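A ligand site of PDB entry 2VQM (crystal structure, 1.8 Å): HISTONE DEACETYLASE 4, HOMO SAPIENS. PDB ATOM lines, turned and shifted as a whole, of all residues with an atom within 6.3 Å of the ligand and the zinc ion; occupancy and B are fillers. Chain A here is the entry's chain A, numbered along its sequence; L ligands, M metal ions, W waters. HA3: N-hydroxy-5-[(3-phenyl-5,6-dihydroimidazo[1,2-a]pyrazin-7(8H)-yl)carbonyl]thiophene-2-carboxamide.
Pro 156 touches the ligand. O of Gly 167 touches CAU of the ligand, 3.5 Å away. Phe 168 touches the ligand. CE2 of Phe 227 touches CAT of the ligand (3.3 Å). CD1 of Leu 299 touches SAS of the ligand (3.8 Å). Gly 330 touches the ligand (CA to OAZ, 3.5 Å). Hydrophobic or aromatic side chains within 4 Å of the ligand: Pro 156, Phe 168, His 198, Phe 227 and Leu 299. Within 4 Å of the ligand: Pro 156, Gly 167, Phe 168, His 198, Phe 227, Asp 290, Leu 299 and Gly 330. The nearest printed residue that does not touch the ligand is His 159 (4.3 Å).
The backbone carbonyl oxygen of Pro 156 is in hydrogen-bond range of the side-chain sulfur of Cys 169, 3.2 Å away. N of Gly 330 sits at hydrogen-bond distance from OD1 of Asp 196, 2.8 Å away. N of Val 197 sits at hydrogen-bond distance from OD1 of Asp 290. O of Leu 299 is in hydrogen-bond range of NE2 of His 198 (3.1 Å). The backbone carbonyl oxygen (O) of Gly 167 is in hydrogen-bond range of the side-chain sulfur (SG) of Cys 169, at 3.6 Å.
The zinc ion is bound by OD2 of Asp 290, water W3, OD2 of Asp 196, ND1 of His 198 and OAY of the ligand. Slightly farther from the zinc ion lies the side-chain carboxylate (OD1) of Asp 196 (2.7 Å).
Water W3 lies within hydrogen-bond range of a ring nitrogen (NE2) of His 158 (2.7 Å), an oxygen (OAZ) of the ligand (3.0 Å), a ring nitrogen (NE2) of His 159 (3.0 Å) and the side-chain carboxylate of Asp 196 (3.2 Å).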
ATOM      1  N   ARG A  37      -1.874   2.575  18.493  1.00  0.00           N
ATOM      2  CA  ARG A  37      -2.926   3.597  18.344  1.00  0.00           C
ATOM      3  C   ARG A  37      -4.334   3.044  18.608  1.00  0.00           C
ATOM      4  O   ARG A  37      -5.021   3.534  19.510  1.00  0.00           O
ATOM      5  CB  ARG A  37      -2.860   4.212  16.945  1.00  0.00           C
ATOM      6  CG  ARG A  37      -1.504   4.774  16.564  1.00  0.00           C
ATOM      7  CD  ARG A  37      -1.311   4.722  15.060  1.00  0.00           C
ATOM      8  NE  ARG A  37      -2.212   5.639  14.403  1.00  0.00           N
ATOM      9  CZ  ARG A  37      -3.091   5.358  13.436  1.00  0.00           C
ATOM     10  NH1 ARG A  37      -3.233   4.155  12.923  1.00  0.00           N
ATOM     11  NH2 ARG A  37      -3.815   6.349  12.952  1.00  0.00           N
ATOM     12  N   PRO A 156      -4.293   3.277   7.922  1.00  0.00           N
ATOM     13  CA  PRO A 156      -5.156   4.165   7.117  1.00  0.00           C
ATOM     14  C   PRO A 156      -5.281   3.711   5.674  1.00  0.00           C
ATOM     15  O   PRO A 156      -4.493   2.875   5.201  1.00  0.00           O
ATOM     16  CB  PRO A 156      -4.439   5.529   7.195  1.00  0.00           C
ATOM     17  CG  PRO A 156      -3.099   5.257   7.683  1.00  0.00           C
ATOM     18  CD  PRO A 156      -3.079   3.952   8.389  1.00  0.00           C
ATOM     19  N   HIS A 158      -6.598   6.183   2.907  1.00  0.00           N
ATOM     20  CA  HIS A 158      -6.928   7.229   1.926  1.00  0.00           C
ATOM     21  C   HIS A 158      -5.850   7.620   0.894  1.00  0.00           C
ATOM     22  O   HIS A 158      -6.172   8.313  -0.098  1.00  0.00           O
ATOM     23  CB  HIS A 158      -7.516   8.479   2.637  1.00  0.00           C
ATOM     24  CG  HIS A 158      -6.518   9.287   3.407  1.00  0.00           C
ATOM     25  ND1 HIS A 158      -6.609  10.658   3.530  1.00  0.00           N
ATOM     26  CD2 HIS A 158      -5.408   8.917   4.087  1.00  0.00           C
ATOM     27  CE1 HIS A 158      -5.601  11.095   4.257  1.00  0.00           C
ATOM     28  NE2 HIS A 158      -4.852  10.059   4.601  1.00  0.00           N
ATOM     29  N   HIS A 159      -4.601   7.196   1.103  1.00  0.00           N
ATOM     30  CA  HIS A 159      -3.542   7.424   0.128  1.00  0.00           C
ATOM     31  C   HIS A 159      -3.397   6.287  -0.891  1.00  0.00           C
ATOM     32  O   HIS A 159      -2.720   6.466  -1.901  1.00  0.00           O
ATOM     33  CB  HIS A 159      -2.174   7.620   0.791  1.00  0.00           C
ATOM     34  CG  HIS A 159      -2.093   8.789   1.714  1.00  0.00           C
ATOM     35  ND1 HIS A 159      -2.433  10.065   1.336  1.00  0.00           N
ATOM     36  CD2 HIS A 159      -1.663   8.877   3.009  1.00  0.00           C
ATOM     37  CE1 HIS A 159      -2.233  10.893   2.357  1.00  0.00           C
ATOM     38  NE2 HIS A 159      -1.761  10.197   3.371  1.00  0.00           N
ATOM     39  N   MET A 166       0.771   3.405  -0.803  1.00  0.00           N
ATOM     40  CA  MET A 166       1.663   4.512  -0.414  1.00  0.00           C
ATOM     41  C   MET A 166       1.209   5.125   0.905  1.00  0.00           C
ATOM     42  O   MET A 166       0.072   4.923   1.347  1.00  0.00           O
ATOM     43  CB  MET A 166       1.733   5.605  -1.489  1.00  0.00           C
ATOM     44  CG  MET A 166       0.401   6.024  -2.084  1.00  0.00           C
ATOM     45  SD  MET A 166       0.513   7.372  -3.285  1.00  0.00           S
ATOM     46  CE  MET A 166       0.842   8.737  -2.188  1.00  0.00           C
ATOM     47  N   GLY A 167       2.121   5.887   1.520  1.00  0.00           N
ATOM     48  CA  GLY A 167       1.844   6.547   2.796  1.00  0.00           C
ATOM     49  C   GLY A 167       1.209   5.658   3.865  1.00  0.00           C
ATOM     50  O   GLY A 167       0.292   6.098   4.562  1.00  0.00           O
ATOM     51  N   PHE A 168       1.712   4.424   3.978  1.00  0.00           N
ATOM     52  CA  PHE A 168       1.280   3.408   4.954  1.00  0.00           C
ATOM     53  C   PHE A 168      -0.078   2.759   4.608  1.00  0.00           C
ATOM     54  O   PHE A 168      -0.557   1.870   5.338  1.00  0.00           O
ATOM     55  CB  PHE A 168       1.281   3.949   6.403  1.00  0.00           C
ATOM     56  CG  PHE A 168       2.596   4.555   6.811  1.00  0.00           C
ATOM     57  CD1 PHE A 168       2.760   5.934   6.864  1.00  0.00           C
ATOM     58  CD2 PHE A 168       3.674   3.747   7.092  1.00  0.00           C
ATOM     59  CE1 PHE A 168       3.983   6.498   7.211  1.00  0.00           C
ATOM     60  CE2 PHE A 168       4.908   4.313   7.448  1.00  0.00           C
ATOM     61  CZ  PHE A 168       5.051   5.688   7.506  1.00  0.00           C
ATOM     62  N   CYS A 169      -0.669   3.146   3.480  1.00  0.00           N
ATOM     63  CA  CYS A 169      -1.980   2.637   3.057  1.00  0.00           C
ATOM     64  C   CYS A 169      -1.853   1.545   1.972  1.00  0.00           C
ATOM     65  O   CYS A 169      -1.152   1.724   0.989  1.00  0.00           O
ATOM     66  CB  CYS A 169      -2.829   3.772   2.470  1.00  0.00           C
ATOM     67  SG  CYS A 169      -3.048   5.179   3.551  1.00  0.00           S
ATOM     68  N   ASP A 196      -8.279  14.403   7.726  1.00  0.00           N
ATOM     69  CA  ASP A 196      -6.888  14.103   7.994  1.00  0.00           C
ATOM     70  C   ASP A 196      -6.065  15.312   7.442  1.00  0.00           C
ATOM     71  O   ASP A 196      -6.453  15.908   6.438  1.00  0.00           O
ATOM     72  CB  ASP A 196      -6.544  12.816   7.258  1.00  0.00           C
ATOM     73  CG  ASP A 196      -5.148  12.320   7.551  1.00  0.00           C
ATOM     74  OD1 ASP A 196      -5.024  11.330   8.322  1.00  0.00           O
ATOM     75  OD2 ASP A 196      -4.199  12.908   6.994  1.00  0.00           O
ATOM     76  N   VAL A 197      -4.967  15.677   8.100  1.00  0.00           N
ATOM     77  CA  VAL A 197      -4.152  16.823   7.636  1.00  0.00           C
ATOM     78  C   VAL A 197      -3.516  16.630   6.224  1.00  0.00           C
ATOM     79  O   VAL A 197      -3.133  17.613   5.564  1.00  0.00           O
ATOM     80  CB  VAL A 197      -3.080  17.192   8.710  1.00  0.00           C
ATOM     81  CG1 VAL A 197      -1.915  16.208   8.673  1.00  0.00           C
ATOM     82  CG2 VAL A 197      -2.627  18.659   8.526  1.00  0.00           C
ATOM     83  N   HIS A 198      -3.438  15.375   5.760  1.00  0.00           N
ATOM     84  CA  HIS A 198      -2.914  15.044   4.433  1.00  0.00           C
ATOM     85  C   HIS A 198      -4.018  14.855   3.391  1.00  0.00           C
ATOM     86  O   HIS A 198      -5.101  14.326   3.708  1.00  0.00           O
ATOM     87  CB  HIS A 198      -2.054  13.776   4.529  1.00  0.00           C
ATOM     88  CG  HIS A 198      -0.943  13.888   5.523  1.00  0.00           C
ATOM     89  ND1 HIS A 198      -0.995  13.294   6.757  1.00  0.00           N
ATOM     90  CD2 HIS A 198       0.249  14.528   5.461  1.00  0.00           C
ATOM     91  CE1 HIS A 198       0.108  13.585   7.427  1.00  0.00           C
ATOM     92  NE2 HIS A 198       0.881  14.323   6.658  1.00  0.00           N
ATOM     93  N   PHE A 226       3.902  19.609   0.712  1.00  0.00           N
ATOM     94  CA  PHE A 226       3.580  18.810   1.911  1.00  0.00           C
ATOM     95  C   PHE A 226       3.057  17.431   1.453  1.00  0.00           C
ATOM     96  O   PHE A 226       2.311  17.360   0.484  1.00  0.00           O
ATOM     97  CB  PHE A 226       2.526  19.555   2.760  1.00  0.00           C
ATOM     98  CG  PHE A 226       2.370  18.997   4.142  1.00  0.00           C
ATOM     99  CD1 PHE A 226       3.398  19.107   5.070  1.00  0.00           C
ATOM    100  CD2 PHE A 226       1.216  18.327   4.508  1.00  0.00           C
ATOM    101  CE1 PHE A 226       3.280  18.552   6.340  1.00  0.00           C
ATOM    102  CE2 PHE A 226       1.076  17.784   5.779  1.00  0.00           C
ATOM    103  CZ  PHE A 226       2.099  17.885   6.692  1.00  0.00           C
ATOM    104  N   PHE A 227       3.455  16.354   2.129  1.00  0.00           N
ATOM    105  CA  PHE A 227       2.994  15.007   1.757  1.00  0.00           C
ATOM    106  C   PHE A 227       1.465  14.913   1.570  1.00  0.00           C
ATOM    107  O   PHE A 227       0.704  15.439   2.419  1.00  0.00           O
ATOM    108  CB  PHE A 227       3.428  13.968   2.801  1.00  0.00           C
ATOM    109  CG  PHE A 227       3.188  12.538   2.375  1.00  0.00           C
ATOM    110  CD1 PHE A 227       4.159  11.852   1.644  1.00  0.00           C
ATOM    111  CD2 PHE A 227       2.002  11.896   2.683  1.00  0.00           C
ATOM    112  CE1 PHE A 227       3.950  10.549   1.230  1.00  0.00           C
ATOM    113  CE2 PHE A 227       1.780  10.578   2.256  1.00  0.00           C
ATOM    114  CZ  PHE A 227       2.776   9.909   1.525  1.00  0.00           C
ATOM    115  N   GLY A 288      -8.881  11.295  10.033  1.00  0.00           N
ATOM    116  CA  GLY A 288      -7.541  11.362  10.625  1.00  0.00           C
ATOM    117  C   GLY A 288      -7.521  12.457  11.657  1.00  0.00           C
ATOM    118  O   GLY A 288      -8.252  13.461  11.532  1.00  0.00           O
ATOM    119  N   ASP A 290      -4.367  13.769  12.715  1.00  0.00           N
ATOM    120  CA  ASP A 290      -3.024  14.353  12.653  1.00  0.00           C
ATOM    121  C   ASP A 290      -2.987  15.900  12.522  1.00  0.00           C
ATOM    122  O   ASP A 290      -1.908  16.487  12.606  1.00  0.00           O
ATOM    123  CB  ASP A 290      -2.086  13.656  11.621  1.00  0.00           C
ATOM    124  CG  ASP A 290      -2.751  13.351  10.265  1.00  0.00           C
ATOM    125  OD1 ASP A 290      -3.853  13.898  10.034  1.00  0.00           O
ATOM    126  OD2 ASP A 290      -2.190  12.554   9.434  1.00  0.00           O
ATOM    127  N   PRO A 298       6.875  18.463  10.440  1.00  0.00           N
ATOM    128  CA  PRO A 298       6.855  17.632   9.220  1.00  0.00           C
ATOM    129  C   PRO A 298       5.665  16.635   9.123  1.00  0.00           C
ATOM    130  O   PRO A 298       5.126  16.435   8.026  1.00  0.00           O
ATOM    131  CB  PRO A 298       8.203  16.887   9.281  1.00  0.00           C
ATOM    132  CG  PRO A 298       8.511  16.812  10.708  1.00  0.00           C
ATOM    133  CD  PRO A 298       7.801  17.941  11.446  1.00  0.00           C
ATOM    134  N   LEU A 299       5.256  16.045  10.247  1.00  0.00           N
ATOM    135  CA  LEU A 299       4.105  15.142  10.306  1.00  0.00           C
ATOM    136  C   LEU A 299       2.766  15.897  10.133  1.00  0.00           C
ATOM    137  O   LEU A 299       1.916  15.482   9.336  1.00  0.00           O
ATOM    138  CB  LEU A 299       4.098  14.363  11.637  1.00  0.00           C
ATOM    139  CG  LEU A 299       3.002  13.308  11.861  1.00  0.00           C
ATOM    140  CD1 LEU A 299       2.844  12.360  10.663  1.00  0.00           C
ATOM    141  CD2 LEU A 299       3.270  12.507  13.149  1.00  0.00           C
ATOM    142  N   GLU A 329      -8.246   7.466  10.091  1.00  0.00           N
ATOM    143  CA  GLU A 329      -7.167   7.444   9.091  1.00  0.00           C
ATOM    144  C   GLU A 329      -5.854   7.680   9.844  1.00  0.00           C
ATOM    145  O   GLU A 329      -5.443   6.820  10.634  1.00  0.00           O
ATOM    146  CB  GLU A 329      -7.416   8.469   7.976  1.00  0.00           C
ATOM    147  CG  GLU A 329      -8.688   8.214   7.145  1.00  0.00           C
ATOM    148  CD  GLU A 329      -8.543   7.202   6.023  1.00  0.00           C
ATOM    149  OE1 GLU A 329      -7.459   6.593   5.836  1.00  0.00           O
ATOM    150  OE2 GLU A 329      -9.549   7.053   5.287  1.00  0.00           O
ATOM    151  N   GLY A 330      -5.212   8.832   9.647  1.00  0.00           N
ATOM    152  CA  GLY A 330      -3.965   9.160  10.359  1.00  0.00           C
ATOM    153  C   GLY A 330      -4.161   9.737  11.745  1.00  0.00           C
ATOM    154  O   GLY A 330      -5.270   9.751  12.275  1.00  0.00           O
ATOM    155  N   GLY A 331      -3.073  10.257  12.327  1.00  0.00           N
ATOM    156  CA  GLY A 331      -3.022  10.593  13.739  1.00  0.00           C
ATOM    157  C   GLY A 331      -2.034   9.655  14.418  1.00  0.00           C
ATOM    158  O   GLY A 331      -2.049   8.454  14.152  1.00  0.00           O
HETATM  159  CAA HA3 L   1      11.837  10.295   6.753  1.00  0.00           C
HETATM  160  CAB HA3 L   1      12.904  11.090   7.191  1.00  0.00           C
HETATM  161  CAC HA3 L   1      12.662  12.346   7.748  1.00  0.00           C
HETATM  162  CAD HA3 L   1      11.349  12.813   7.871  1.00  0.00           C
HETATM  163  CAE HA3 L   1      10.290  12.024   7.432  1.00  0.00           C
HETATM  164  CAF HA3 L   1      10.521  10.749   6.870  1.00  0.00           C
HETATM  165  CAG HA3 L   1       9.473   9.946   6.400  1.00  0.00           C
HETATM  166  CAH HA3 L   1       9.418   8.609   6.233  1.00  0.00           C
HETATM  167  NAI HA3 L   1       8.228   8.262   5.722  1.00  0.00           N
HETATM  168  CAJ HA3 L   1       7.472   9.338   5.523  1.00  0.00           C
HETATM  169  CAK HA3 L   1       6.023   9.456   4.954  1.00  0.00           C
HETATM  170  NAL HA3 L   1       8.249  10.449   5.948  1.00  0.00           N
HETATM  171  CAM HA3 L   1       7.754  11.825   5.885  1.00  0.00           C
HETATM  172  CAN HA3 L   1       6.694  11.884   4.837  1.00  0.00           C
HETATM  173  NAO HA3 L   1       5.658  10.881   5.135  1.00  0.00           N
HETATM  174  CAP HA3 L   1       4.535  11.359   5.648  1.00  0.00           C
HETATM  175  OAQ HA3 L   1       4.426  12.583   5.780  1.00  0.00           O
HETATM  176  CAR HA3 L   1       3.314  10.559   5.965  1.00  0.00           C
HETATM  177  SAS HA3 L   1       2.198  11.036   7.109  1.00  0.00           S
HETATM  178  CAT HA3 L   1       2.852   9.534   5.250  1.00  0.00           C
HETATM  179  CAU HA3 L   1       1.650   9.081   5.680  1.00  0.00           C
HETATM  180  CAV HA3 L   1       1.159   9.791   6.701  1.00  0.00           C
HETATM  181  CAW HA3 L   1      -0.167   9.534   7.401  1.00  0.00           C
HETATM  182  OAY HA3 L   1      -0.620  10.406   8.155  1.00  0.00           O
HETATM  183  NAX HA3 L   1      -0.762   8.368   7.137  1.00  0.00           N
HETATM  184  OAZ HA3 L   1      -1.949   8.075   7.725  1.00  0.00           O
HETATM  185 ZN    ZN M   1      -2.456  12.003   7.616  1.00  0.00          ZN
HETATM  186  O   HOH W   1       3.595  14.945   6.430  1.00  0.00           O
HETATM  187  O   HOH W   2      -0.532  10.472  11.155  1.00  0.00           O
HETATM  188  O   HOH W   3      -2.764  10.533   6.230  1.00  0.00           O
HETATM  189  O   HOH W   4       7.522   6.193   4.481  1.00  0.00           O
